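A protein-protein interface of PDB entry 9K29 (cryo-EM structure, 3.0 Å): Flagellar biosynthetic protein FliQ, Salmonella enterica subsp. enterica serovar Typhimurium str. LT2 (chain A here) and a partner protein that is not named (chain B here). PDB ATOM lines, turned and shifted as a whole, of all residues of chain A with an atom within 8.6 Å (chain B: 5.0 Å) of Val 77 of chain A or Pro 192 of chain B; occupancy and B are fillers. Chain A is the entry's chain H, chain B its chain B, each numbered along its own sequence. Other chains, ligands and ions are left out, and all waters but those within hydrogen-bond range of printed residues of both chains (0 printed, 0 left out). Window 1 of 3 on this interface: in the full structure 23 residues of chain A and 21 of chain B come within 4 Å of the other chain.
The backbone carbonyl oxygen (O) of Arg 78 of chain A lies within hydrogen-bond range of the side-chain hydroxyl (OG) of Ser 82 of chain A (3.1 Å).
Of chain B, only Pro 192 (3.9 Å), Leu 225 (3.7 Å) and Val 229 (3.6 Å) come within 4 Å of Val 77 of chain A. Of the printed residues of chain B, Leu 84 of chain A touches Thr 188. Of the printed residues of chain B, Leu 74 of chain A touches Val 229. Printed residues of chain B within 4 Å of Ala 13 of chain A: Ile 191 and Ile 195. Printed residues of chain B within 4 Å of Met 9 of chain A: Ile 191 (3.5 Å). Of the printed residues of chain B, Arg 78 of chain A touches Val 229. Phe 190 of chain B touches none of the printed residues of chain A. Asn 71 of chain A touches none of the printed residues of chain B. The nearest printed residue of chain B that does not touch Val 77 of chain A is Phe 193 of chain B (6.8 Å). The nearest printed residue of chain B that does not touch Leu 73 of chain A is Ile 196 of chain B (4.2 Å).
Hydrophobic or aromatic side chains of chain A within 4 Å of the printed part of chain B: Met 9, Ala 13, Ala 17, Leu 20, Leu 73, Leu 74, Tyr 76, Val 77, Leu 80 and Leu 84. Among the printed residues, 16 pairs touch across the chains. Among the printed residues, no Asp or Glu carboxylate lies within 4 Å of a Lys or Arg side-chain nitrogen of the other chain.
Among the printed residues, pairs that only touch across the chains: Tyr 76 of chain A with Ile 191 of chain B (3.2 Å), Leu 80 of chain A with Thr 188 of chain B (3.4 Å), Ala 13 of chain A with Ile 195 of chain B (3.4 Å), Met 9 of chain A with Ile 191 of chain B (3.5 Å), Arg 78 of chain A with Val 229 of chain B (3.5 Å), Val 77 of chain A with Val 229 of chain B (3.6 Å), Leu 73 of chain A with Leu 225 of chain B (3.6 Å), Ala 13 of chain A with Ile 191 of chain B (3.6 Å), Ala 17 of chain A with Ile 195 of chain B (3.6 Å), Leu 84 of chain A with Thr 188 of chain B (3.6 Å), Tyr 76 of chain A with Ile 195 of chain B (3.7 Å), Val 77 of chain A with Leu 225 of chain B (3.7 Å), Leu 80 of chain A with Pro 192 of chain B (3.8 Å), Leu 74 of chain A with Val 229 of chain B (3.8 Å), Val 77 of chain A with Pro 192 of chain B (3.9 Å) and Leu 20 of chain A with Ile 195 of chain B (3.998 Å).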
ATOM      1  N   MET A   9       3.127  19.989   7.364  1.00  0.00           N
ATOM      2  CA  MET A   9       3.277  20.487   8.727  1.00  0.00           C
ATOM      3  C   MET A   9       2.621  21.853   8.890  1.00  0.00           C
ATOM      4  O   MET A   9       1.948  22.113   9.895  1.00  0.00           O
ATOM      5  CB  MET A   9       4.763  20.547   9.080  1.00  0.00           C
ATOM      6  CG  MET A   9       5.092  21.194  10.407  1.00  0.00           C
ATOM      7  SD  MET A   9       6.846  21.602  10.504  1.00  0.00           S
ATOM      8  CE  MET A   9       7.595  20.039  10.054  1.00  0.00           C
ATOM      9  N   GLU A  12      -1.189  21.476   8.907  1.00  0.00           N
ATOM     10  CA  GLU A  12      -1.634  20.938  10.190  1.00  0.00           C
ATOM     11  C   GLU A  12      -1.568  22.006  11.280  1.00  0.00           C
ATOM     12  O   GLU A  12      -2.466  22.102  12.130  1.00  0.00           O
ATOM     13  CB  GLU A  12      -0.793  19.713  10.549  1.00  0.00           C
ATOM     14  CG  GLU A  12      -1.292  18.910  11.739  1.00  0.00           C
ATOM     15  CD  GLU A  12      -0.830  19.481  13.055  1.00  0.00           C
ATOM     16  OE1 GLU A  12       0.248  20.108  13.071  1.00  0.00           O
ATOM     17  OE2 GLU A  12      -1.532  19.294  14.070  1.00  0.00           O
ATOM     18  N   ALA A  13      -0.519  22.832  11.260  1.00  0.00           N
ATOM     19  CA  ALA A  13      -0.418  23.928  12.220  1.00  0.00           C
ATOM     20  C   ALA A  13      -1.538  24.944  12.025  1.00  0.00           C
ATOM     21  O   ALA A  13      -2.093  25.460  13.000  1.00  0.00           O
ATOM     22  CB  ALA A  13       0.946  24.606  12.099  1.00  0.00           C
ATOM     23  N   VAL A  16      -4.630  23.553  13.542  1.00  0.00           N
ATOM     24  CA  VAL A  16      -4.630  23.725  14.995  1.00  0.00           C
ATOM     25  C   VAL A  16      -4.960  25.166  15.365  1.00  0.00           C
ATOM     26  O   VAL A  16      -5.756  25.423  16.277  1.00  0.00           O
ATOM     27  CB  VAL A  16      -3.280  23.285  15.589  1.00  0.00           C
ATOM     28  CG1 VAL A  16      -3.243  23.565  17.081  1.00  0.00           C
ATOM     29  CG2 VAL A  16      -3.047  21.812  15.324  1.00  0.00           C
ATOM     30  N   ALA A  17      -4.355  26.128  14.664  1.00  0.00           N
ATOM     31  CA  ALA A  17      -4.607  27.536  14.957  1.00  0.00           C
ATOM     32  C   ALA A  17      -6.064  27.902  14.708  1.00  0.00           C
ATOM     33  O   ALA A  17      -6.671  28.636  15.497  1.00  0.00           O
ATOM     34  CB  ALA A  17      -3.683  28.420  14.118  1.00  0.00           C
ATOM     35  N   LEU A  20      -8.174  26.556  17.437  1.00  0.00           N
ATOM     36  CA  LEU A  20      -8.022  27.395  18.622  1.00  0.00           C
ATOM     37  C   LEU A  20      -8.838  28.677  18.506  1.00  0.00           C
ATOM     38  O   LEU A  20      -9.454  29.117  19.483  1.00  0.00           O
ATOM     39  CB  LEU A  20      -6.548  27.726  18.845  1.00  0.00           C
ATOM     40  CG  LEU A  20      -5.645  26.614  19.377  1.00  0.00           C
ATOM     41  CD1 LEU A  20      -4.271  27.164  19.721  1.00  0.00           C
ATOM     42  CD2 LEU A  20      -6.272  25.947  20.584  1.00  0.00           C
ATOM     43  N   LEU A  70      -7.176  23.594  25.259  1.00  0.00           N
ATOM     44  CA  LEU A  70      -5.932  23.332  25.975  1.00  0.00           C
ATOM     45  C   LEU A  70      -5.409  21.933  25.678  1.00  0.00           C
ATOM     46  O   LEU A  70      -4.219  21.755  25.393  1.00  0.00           O
ATOM     47  CB  LEU A  70      -6.137  23.520  27.477  1.00  0.00           C
ATOM     48  CG  LEU A  70      -4.857  23.648  28.305  1.00  0.00           C
ATOM     49  CD1 LEU A  70      -3.988  24.775  27.775  1.00  0.00           C
ATOM     50  CD2 LEU A  70      -5.186  23.865  29.772  1.00  0.00           C
ATOM     51  N   ASN A  71      -6.287  20.928  25.720  1.00  0.00           N
ATOM     52  CA  ASN A  71      -5.871  19.559  25.441  1.00  0.00           C
ATOM     53  C   ASN A  71      -5.416  19.404  23.998  1.00  0.00           C
ATOM     54  O   ASN A  71      -4.418  18.728  23.727  1.00  0.00           O
ATOM     55  CB  ASN A  71      -7.012  18.591  25.749  1.00  0.00           C
ATOM     56  CG  ASN A  71      -7.238  18.412  27.236  1.00  0.00           C
ATOM     57  OD1 ASN A  71      -6.313  18.547  28.035  1.00  0.00           O
ATOM     58  ND2 ASN A  71      -8.473  18.107  27.614  1.00  0.00           N
ATOM     59  N   LEU A  72      -6.135  20.020  23.056  1.00  0.00           N
ATOM     60  CA  LEU A  72      -5.736  19.936  21.654  1.00  0.00           C
ATOM     61  C   LEU A  72      -4.346  20.525  21.446  1.00  0.00           C
ATOM     62  O   LEU A  72      -3.484  19.910  20.802  1.00  0.00           O
ATOM     63  CB  LEU A  72      -6.761  20.651  20.776  1.00  0.00           C
ATOM     64  CG  LEU A  72      -6.533  20.567  19.268  1.00  0.00           C
ATOM     65  CD1 LEU A  72      -7.096  19.270  18.713  1.00  0.00           C
ATOM     66  CD2 LEU A  72      -7.151  21.766  18.572  1.00  0.00           C
ATOM     67  N   LEU A  73      -4.107  21.715  21.998  1.00  0.00           N
ATOM     68  CA  LEU A  73      -2.812  22.364  21.829  1.00  0.00           C
ATOM     69  C   LEU A  73      -1.701  21.566  22.502  1.00  0.00           C
ATOM     70  O   LEU A  73      -0.609  21.415  21.941  1.00  0.00           O
ATOM     71  CB  LEU A  73      -2.874  23.787  22.381  1.00  0.00           C
ATOM     72  CG  LEU A  73      -1.659  24.683  22.162  1.00  0.00           C
ATOM     73  CD1 LEU A  73      -1.390  24.864  20.680  1.00  0.00           C
ATOM     74  CD2 LEU A  73      -1.894  26.027  22.827  1.00  0.00           C
ATOM     75  N   LEU A  74      -1.961  21.044  23.704  1.00  0.00           N
ATOM     76  CA  LEU A  74      -0.947  20.253  24.394  1.00  0.00           C
ATOM     77  C   LEU A  74      -0.612  18.985  23.622  1.00  0.00           C
ATOM     78  O   LEU A  74       0.561  18.619  23.504  1.00  0.00           O
ATOM     79  CB  LEU A  74      -1.409  19.915  25.810  1.00  0.00           C
ATOM     80  CG  LEU A  74      -1.464  21.080  26.798  1.00  0.00           C
ATOM     81  CD1 LEU A  74      -1.992  20.614  28.144  1.00  0.00           C
ATOM     82  CD2 LEU A  74      -0.094  21.720  26.946  1.00  0.00           C
ATOM     83  N   ASP A  75      -1.627  18.296  23.094  1.00  0.00           N
ATOM     84  CA  ASP A  75      -1.367  17.093  22.308  1.00  0.00           C
ATOM     85  C   ASP A  75      -0.576  17.421  21.050  1.00  0.00           C
ATOM     86  O   ASP A  75       0.343  16.681  20.674  1.00  0.00           O
ATOM     87  CB  ASP A  75      -2.681  16.399  21.953  1.00  0.00           C
ATOM     88  CG  ASP A  75      -3.442  15.933  23.178  1.00  0.00           C
ATOM     89  OD1 ASP A  75      -2.807  15.740  24.235  1.00  0.00           O
ATOM     90  OD2 ASP A  75      -4.675  15.762  23.084  1.00  0.00           O
ATOM     91  N   TYR A  76      -0.918  18.528  20.386  1.00  0.00           N
ATOM     92  CA  TYR A  76      -0.169  18.928  19.200  1.00  0.00           C
ATOM     93  C   TYR A  76       1.293  19.202  19.535  1.00  0.00           C
ATOM     94  O   TYR A  76       2.196  18.765  18.811  1.00  0.00           O
ATOM     95  CB  TYR A  76      -0.813  20.160  18.564  1.00  0.00           C
ATOM     96  CG  TYR A  76       0.092  20.889  17.600  1.00  0.00           C
ATOM     97  CD1 TYR A  76       0.657  20.233  16.517  1.00  0.00           C
ATOM     98  CD2 TYR A  76       0.384  22.234  17.776  1.00  0.00           C
ATOM     99  CE1 TYR A  76       1.488  20.893  15.642  1.00  0.00           C
ATOM    100  CE2 TYR A  76       1.211  22.904  16.900  1.00  0.00           C
ATOM    101  CZ  TYR A  76       1.759  22.227  15.834  1.00  0.00           C
ATOM    102  OH  TYR A  76       2.585  22.881  14.953  1.00  0.00           O
ATOM    103  N   VAL A  77       1.547  19.919  20.632  1.00  0.00           N
ATOM    104  CA  VAL A  77       2.925  20.242  20.990  1.00  0.00           C
ATOM    105  C   VAL A  77       3.685  18.984  21.399  1.00  0.00           C
ATOM    106  O   VAL A  77       4.869  18.830  21.077  1.00  0.00           O
ATOM    107  CB  VAL A  77       2.957  21.319  22.090  1.00  0.00           C
ATOM    108  CG1 VAL A  77       4.386  21.591  22.522  1.00  0.00           C
ATOM    109  CG2 VAL A  77       2.316  22.598  21.586  1.00  0.00           C
ATOM    110  N   ARG A  78       3.023  18.064  22.108  1.00  0.00           N
ATOM    111  CA  ARG A  78       3.667  16.800  22.458  1.00  0.00           C
ATOM    112  C   ARG A  78       4.056  16.023  21.210  1.00  0.00           C
ATOM    113  O   ARG A  78       5.171  15.501  21.113  1.00  0.00           O
ATOM    114  CB  ARG A  78       2.748  15.952  23.339  1.00  0.00           C
ATOM    115  CG  ARG A  78       2.488  16.515  24.718  1.00  0.00           C
ATOM    116  CD  ARG A  78       1.600  15.598  25.537  1.00  0.00           C
ATOM    117  NE  ARG A  78       1.275  16.180  26.833  1.00  0.00           N
ATOM    118  CZ  ARG A  78       2.009  16.028  27.926  1.00  0.00           C
ATOM    119  NH1 ARG A  78       3.125  15.318  27.915  1.00  0.00           N
ATOM    120  NH2 ARG A  78       1.615  16.605  29.057  1.00  0.00           N
ATOM    121  N   THR A  79       3.144  15.939  20.237  1.00  0.00           N
ATOM    122  CA  THR A  79       3.451  15.223  19.004  1.00  0.00           C
ATOM    123  C   THR A  79       4.602  15.885  18.257  1.00  0.00           C
ATOM    124  O   THR A  79       5.503  15.201  17.755  1.00  0.00           O
ATOM    125  CB  THR A  79       2.207  15.148  18.118  1.00  0.00           C
ATOM    126  OG1 THR A  79       1.166  14.450  18.812  1.00  0.00           O
ATOM    127  CG2 THR A  79       2.518  14.419  16.822  1.00  0.00           C
ATOM    128  N   LEU A  80       4.593  17.218  18.184  1.00  0.00           N
ATOM    129  CA  LEU A  80       5.658  17.927  17.483  1.00  0.00           C
ATOM    130  C   LEU A  80       7.010  17.700  18.149  1.00  0.00           C
ATOM    131  O   LEU A  80       8.006  17.422  17.471  1.00  0.00           O
ATOM    132  CB  LEU A  80       5.334  19.418  17.417  1.00  0.00           C
ATOM    133  CG  LEU A  80       6.074  20.233  16.357  1.00  0.00           C
ATOM    134  CD1 LEU A  80       5.613  19.835  14.966  1.00  0.00           C
ATOM    135  CD2 LEU A  80       5.863  21.717  16.590  1.00  0.00           C
ATOM    136  N   PHE A  81       7.064  17.793  19.478  1.00  0.00           N
ATOM    137  CA  PHE A  81       8.336  17.621  20.169  1.00  0.00           C
ATOM    138  C   PHE A  81       8.785  16.166  20.173  1.00  0.00           C
ATOM    139  O   PHE A  81       9.984  15.890  20.284  1.00  0.00           O
ATOM    140  CB  PHE A  81       8.238  18.158  21.596  1.00  0.00           C
ATOM    141  CG  PHE A  81       8.271  19.659  21.683  1.00  0.00           C
ATOM    142  CD1 PHE A  81       8.401  20.431  20.542  1.00  0.00           C
ATOM    143  CD2 PHE A  81       8.171  20.297  22.908  1.00  0.00           C
ATOM    144  CE1 PHE A  81       8.429  21.810  20.619  1.00  0.00           C
ATOM    145  CE2 PHE A  81       8.201  21.676  22.991  1.00  0.00           C
ATOM    146  CZ  PHE A  81       8.330  22.433  21.845  1.00  0.00           C
ATOM    147  N   SER A  82       7.848  15.222  20.058  1.00  0.00           N
ATOM    148  CA  SER A  82       8.229  13.819  19.965  1.00  0.00           C
ATOM    149  C   SER A  82       8.763  13.484  18.577  1.00  0.00           C
ATOM    150  O   SER A  82       9.669  12.656  18.440  1.00  0.00           O
ATOM    151  CB  SER A  82       7.038  12.927  20.314  1.00  0.00           C
ATOM    152  OG  SER A  82       6.787  12.938  21.708  1.00  0.00           O
ATOM    153  N   ASN A  83       8.211  14.109  17.541  1.00  0.00           N
ATOM    154  CA  ASN A  83       8.685  13.898  16.179  1.00  0.00           C
ATOM    155  C   ASN A  83       9.864  14.793  15.817  1.00  0.00           C
ATOM    156  O   ASN A  83      10.423  14.644  14.725  1.00  0.00           O
ATOM    157  CB  ASN A  83       7.544  14.121  15.183  1.00  0.00           C
ATOM    158  CG  ASN A  83       6.383  13.174  15.411  1.00  0.00           C
ATOM    159  OD1 ASN A  83       6.344  12.450  16.405  1.00  0.00           O
ATOM    160  ND2 ASN A  83       5.429  13.174  14.487  1.00  0.00           N
ATOM    161  N   LEU A  84      10.238  15.722  16.696  1.00  0.00           N
ATOM    162  CA  LEU A  84      11.404  16.569  16.446  1.00  0.00           C
ATOM    163  C   LEU A  84      12.673  15.789  16.120  1.00  0.00           C
ATOM    164  O   LEU A  84      13.349  16.145  15.138  1.00  0.00           O
ATOM    165  CB  LEU A  84      11.621  17.497  17.645  1.00  0.00           C
ATOM    166  CG  LEU A  84      12.636  18.626  17.472  1.00  0.00           C
ATOM    167  CD1 LEU A  84      12.212  19.556  16.355  1.00  0.00           C
ATOM    168  CD2 LEU A  84      12.804  19.391  18.773  1.00  0.00           C
ATOM    169  N   THR B 188      11.010  24.316  13.614  1.00  0.00           N
ATOM    170  CA  THR B 188       9.962  23.479  14.189  1.00  0.00           C
ATOM    171  C   THR B 188       9.533  23.993  15.559  1.00  0.00           C
ATOM    172  O   THR B 188       8.354  23.891  15.919  1.00  0.00           O
ATOM    173  CB  THR B 188      10.440  22.031  14.284  1.00  0.00           C
ATOM    174  OG1 THR B 188      10.848  21.578  12.988  1.00  0.00           O
ATOM    175  CG2 THR B 188       9.324  21.131  14.787  1.00  0.00           C
ATOM    176  N   ILE B 189      10.468  24.557  16.324  1.00  0.00           N
ATOM    177  CA  ILE B 189      10.149  25.054  17.661  1.00  0.00           C
ATOM    178  C   ILE B 189       9.254  26.287  17.587  1.00  0.00           C
ATOM    179  O   ILE B 189       8.307  26.428  18.371  1.00  0.00           O
ATOM    180  CB  ILE B 189      11.447  25.337  18.438  1.00  0.00           C
ATOM    181  CG1 ILE B 189      12.014  24.040  19.015  1.00  0.00           C
ATOM    182  CG2 ILE B 189      11.209  26.350  19.545  1.00  0.00           C
ATOM    183  CD1 ILE B 189      13.322  24.226  19.744  1.00  0.00           C
ATOM    184  N   PHE B 190       9.538  27.203  16.655  1.00  0.00           N
ATOM    185  CA  PHE B 190       8.758  28.441  16.571  1.00  0.00           C
ATOM    186  C   PHE B 190       7.270  28.216  16.329  1.00  0.00           C
ATOM    187  O   PHE B 190       6.466  29.084  16.687  1.00  0.00           O
ATOM    188  CB  PHE B 190       9.272  29.373  15.466  1.00  0.00           C
ATOM    189  CG  PHE B 190      10.567  30.061  15.784  1.00  0.00           C
ATOM    190  CD1 PHE B 190      10.577  31.191  16.580  1.00  0.00           C
ATOM    191  CD2 PHE B 190      11.759  29.624  15.247  1.00  0.00           C
ATOM    192  CE1 PHE B 190      11.757  31.845  16.865  1.00  0.00           C
ATOM    193  CE2 PHE B 190      12.942  30.269  15.536  1.00  0.00           C
ATOM    194  CZ  PHE B 190      12.941  31.383  16.341  1.00  0.00           C
ATOM    195  N   ILE B 191       6.881  27.090  15.729  1.00  0.00           N
ATOM    196  CA  ILE B 191       5.520  26.969  15.200  1.00  0.00           C
ATOM    197  C   ILE B 191       4.446  27.080  16.278  1.00  0.00           C
ATOM    198  O   ILE B 191       3.505  27.870  16.096  1.00  0.00           O
ATOM    199  CB  ILE B 191       5.392  25.684  14.363  1.00  0.00           C
ATOM    200  CG1 ILE B 191       6.342  25.746  13.171  1.00  0.00           C
ATOM    201  CG2 ILE B 191       3.972  25.512  13.876  1.00  0.00           C
ATOM    202  CD1 ILE B 191       6.388  24.479  12.381  1.00  0.00           C
ATOM    203  N   PRO B 192       4.497  26.333  17.391  1.00  0.00           N
ATOM    204  CA  PRO B 192       3.443  26.511  18.409  1.00  0.00           C
ATOM    205  C   PRO B 192       3.389  27.914  18.989  1.00  0.00           C
ATOM    206  O   PRO B 192       2.297  28.439  19.246  1.00  0.00           O
ATOM    207  CB  PRO B 192       3.803  25.465  19.474  1.00  0.00           C
ATOM    208  CG  PRO B 192       5.235  25.152  19.241  1.00  0.00           C
ATOM    209  CD  PRO B 192       5.426  25.255  17.767  1.00  0.00           C
ATOM    210  N   PHE B 193       4.546  28.548  19.188  1.00  0.00           N
ATOM    211  CA  PHE B 193       4.558  29.908  19.712  1.00  0.00           C
ATOM    212  C   PHE B 193       4.002  30.892  18.692  1.00  0.00           C
ATOM    213  O   PHE B 193       3.299  31.844  19.053  1.00  0.00           O
ATOM    214  CB  PHE B 193       5.977  30.287  20.128  1.00  0.00           C
ATOM    215  CG  PHE B 193       6.562  29.370  21.162  1.00  0.00           C
ATOM    216  CD1 PHE B 193       5.806  28.957  22.246  1.00  0.00           C
ATOM    217  CD2 PHE B 193       7.858  28.907  21.042  1.00  0.00           C
ATOM    218  CE1 PHE B 193       6.339  28.109  23.195  1.00  0.00           C
ATOM    219  CE2 PHE B 193       8.396  28.058  21.988  1.00  0.00           C
ATOM    220  CZ  PHE B 193       7.636  27.659  23.066  1.00  0.00           C
ATOM    221  N   LEU B 194       4.296  30.669  17.409  1.00  0.00           N
ATOM    222  CA  LEU B 194       3.693  31.483  16.360  1.00  0.00           C
ATOM    223  C   LEU B 194       2.180  31.318  16.344  1.00  0.00           C
ATOM    224  O   LEU B 194       1.443  32.294  16.160  1.00  0.00           O
ATOM    225  CB  LEU B 194       4.286  31.113  15.003  1.00  0.00           C
ATOM    226  CG  LEU B 194       4.058  32.120  13.878  1.00  0.00           C
ATOM    227  CD1 LEU B 194       4.829  33.397  14.154  1.00  0.00           C
ATOM    228  CD2 LEU B 194       4.454  31.527  12.537  1.00  0.00           C
ATOM    229  N   ILE B 195       1.700  30.087  16.531  1.00  0.00           N
ATOM    230  CA  ILE B 195       0.261  29.844  16.594  1.00  0.00           C
ATOM    231  C   ILE B 195      -0.357  30.602  17.760  1.00  0.00           C
ATOM    232  O   ILE B 195      -1.404  31.244  17.615  1.00  0.00           O
ATOM    233  CB  ILE B 195      -0.022  28.333  16.691  1.00  0.00           C
ATOM    234  CG1 ILE B 195       0.403  27.623  15.406  1.00  0.00           C
ATOM    235  CG2 ILE B 195      -1.487  28.078  17.001  1.00  0.00           C
ATOM    236  CD1 ILE B 195       0.171  26.131  15.434  1.00  0.00           C
ATOM    237  N   ILE B 196       0.278  30.539  18.932  1.00  0.00           N
ATOM    238  CA  ILE B 196      -0.248  31.238  20.102  1.00  0.00           C
ATOM    239  C   ILE B 196      -0.305  32.738  19.842  1.00  0.00           C
ATOM    240  O   ILE B 196      -1.314  33.399  20.119  1.00  0.00           O
ATOM    241  CB  ILE B 196       0.597  30.916  21.348  1.00  0.00           C
ATOM    242  CG1 ILE B 196       0.284  29.512  21.860  1.00  0.00           C
ATOM    243  CG2 ILE B 196       0.356  31.944  22.440  1.00  0.00           C
ATOM    244  CD1 ILE B 196       1.066  29.143  23.094  1.00  0.00           C
ATOM    245  N   LEU B 225       2.014  26.951  28.309  1.00  0.00           N
ATOM    246  CA  LEU B 225       2.228  25.830  27.403  1.00  0.00           C
ATOM    247  C   LEU B 225       3.539  25.120  27.692  1.00  0.00           C
ATOM    248  O   LEU B 225       3.565  23.891  27.800  1.00  0.00           O
ATOM    249  CB  LEU B 225       2.196  26.310  25.948  1.00  0.00           C
ATOM    250  CG  LEU B 225       2.402  25.273  24.838  1.00  0.00           C
ATOM    251  CD1 LEU B 225       1.584  25.640  23.624  1.00  0.00           C
ATOM    252  CD2 LEU B 225       3.870  25.160  24.439  1.00  0.00           C
ATOM    253  N   VAL B 229       3.187  21.201  28.816  1.00  0.00           N
ATOM    254  CA  VAL B 229       3.652  20.149  27.922  1.00  0.00           C
ATOM    255  C   VAL B 229       4.937  19.513  28.428  1.00  0.00           C
ATOM    256  O   VAL B 229       5.436  18.561  27.812  1.00  0.00           O
ATOM    257  CB  VAL B 229       3.859  20.705  26.496  1.00  0.00           C
ATOM    258  CG1 VAL B 229       5.089  21.597  26.435  1.00  0.00           C
ATOM    259  CG2 VAL B 229       3.925  19.594  25.464  1.00  0.00           C
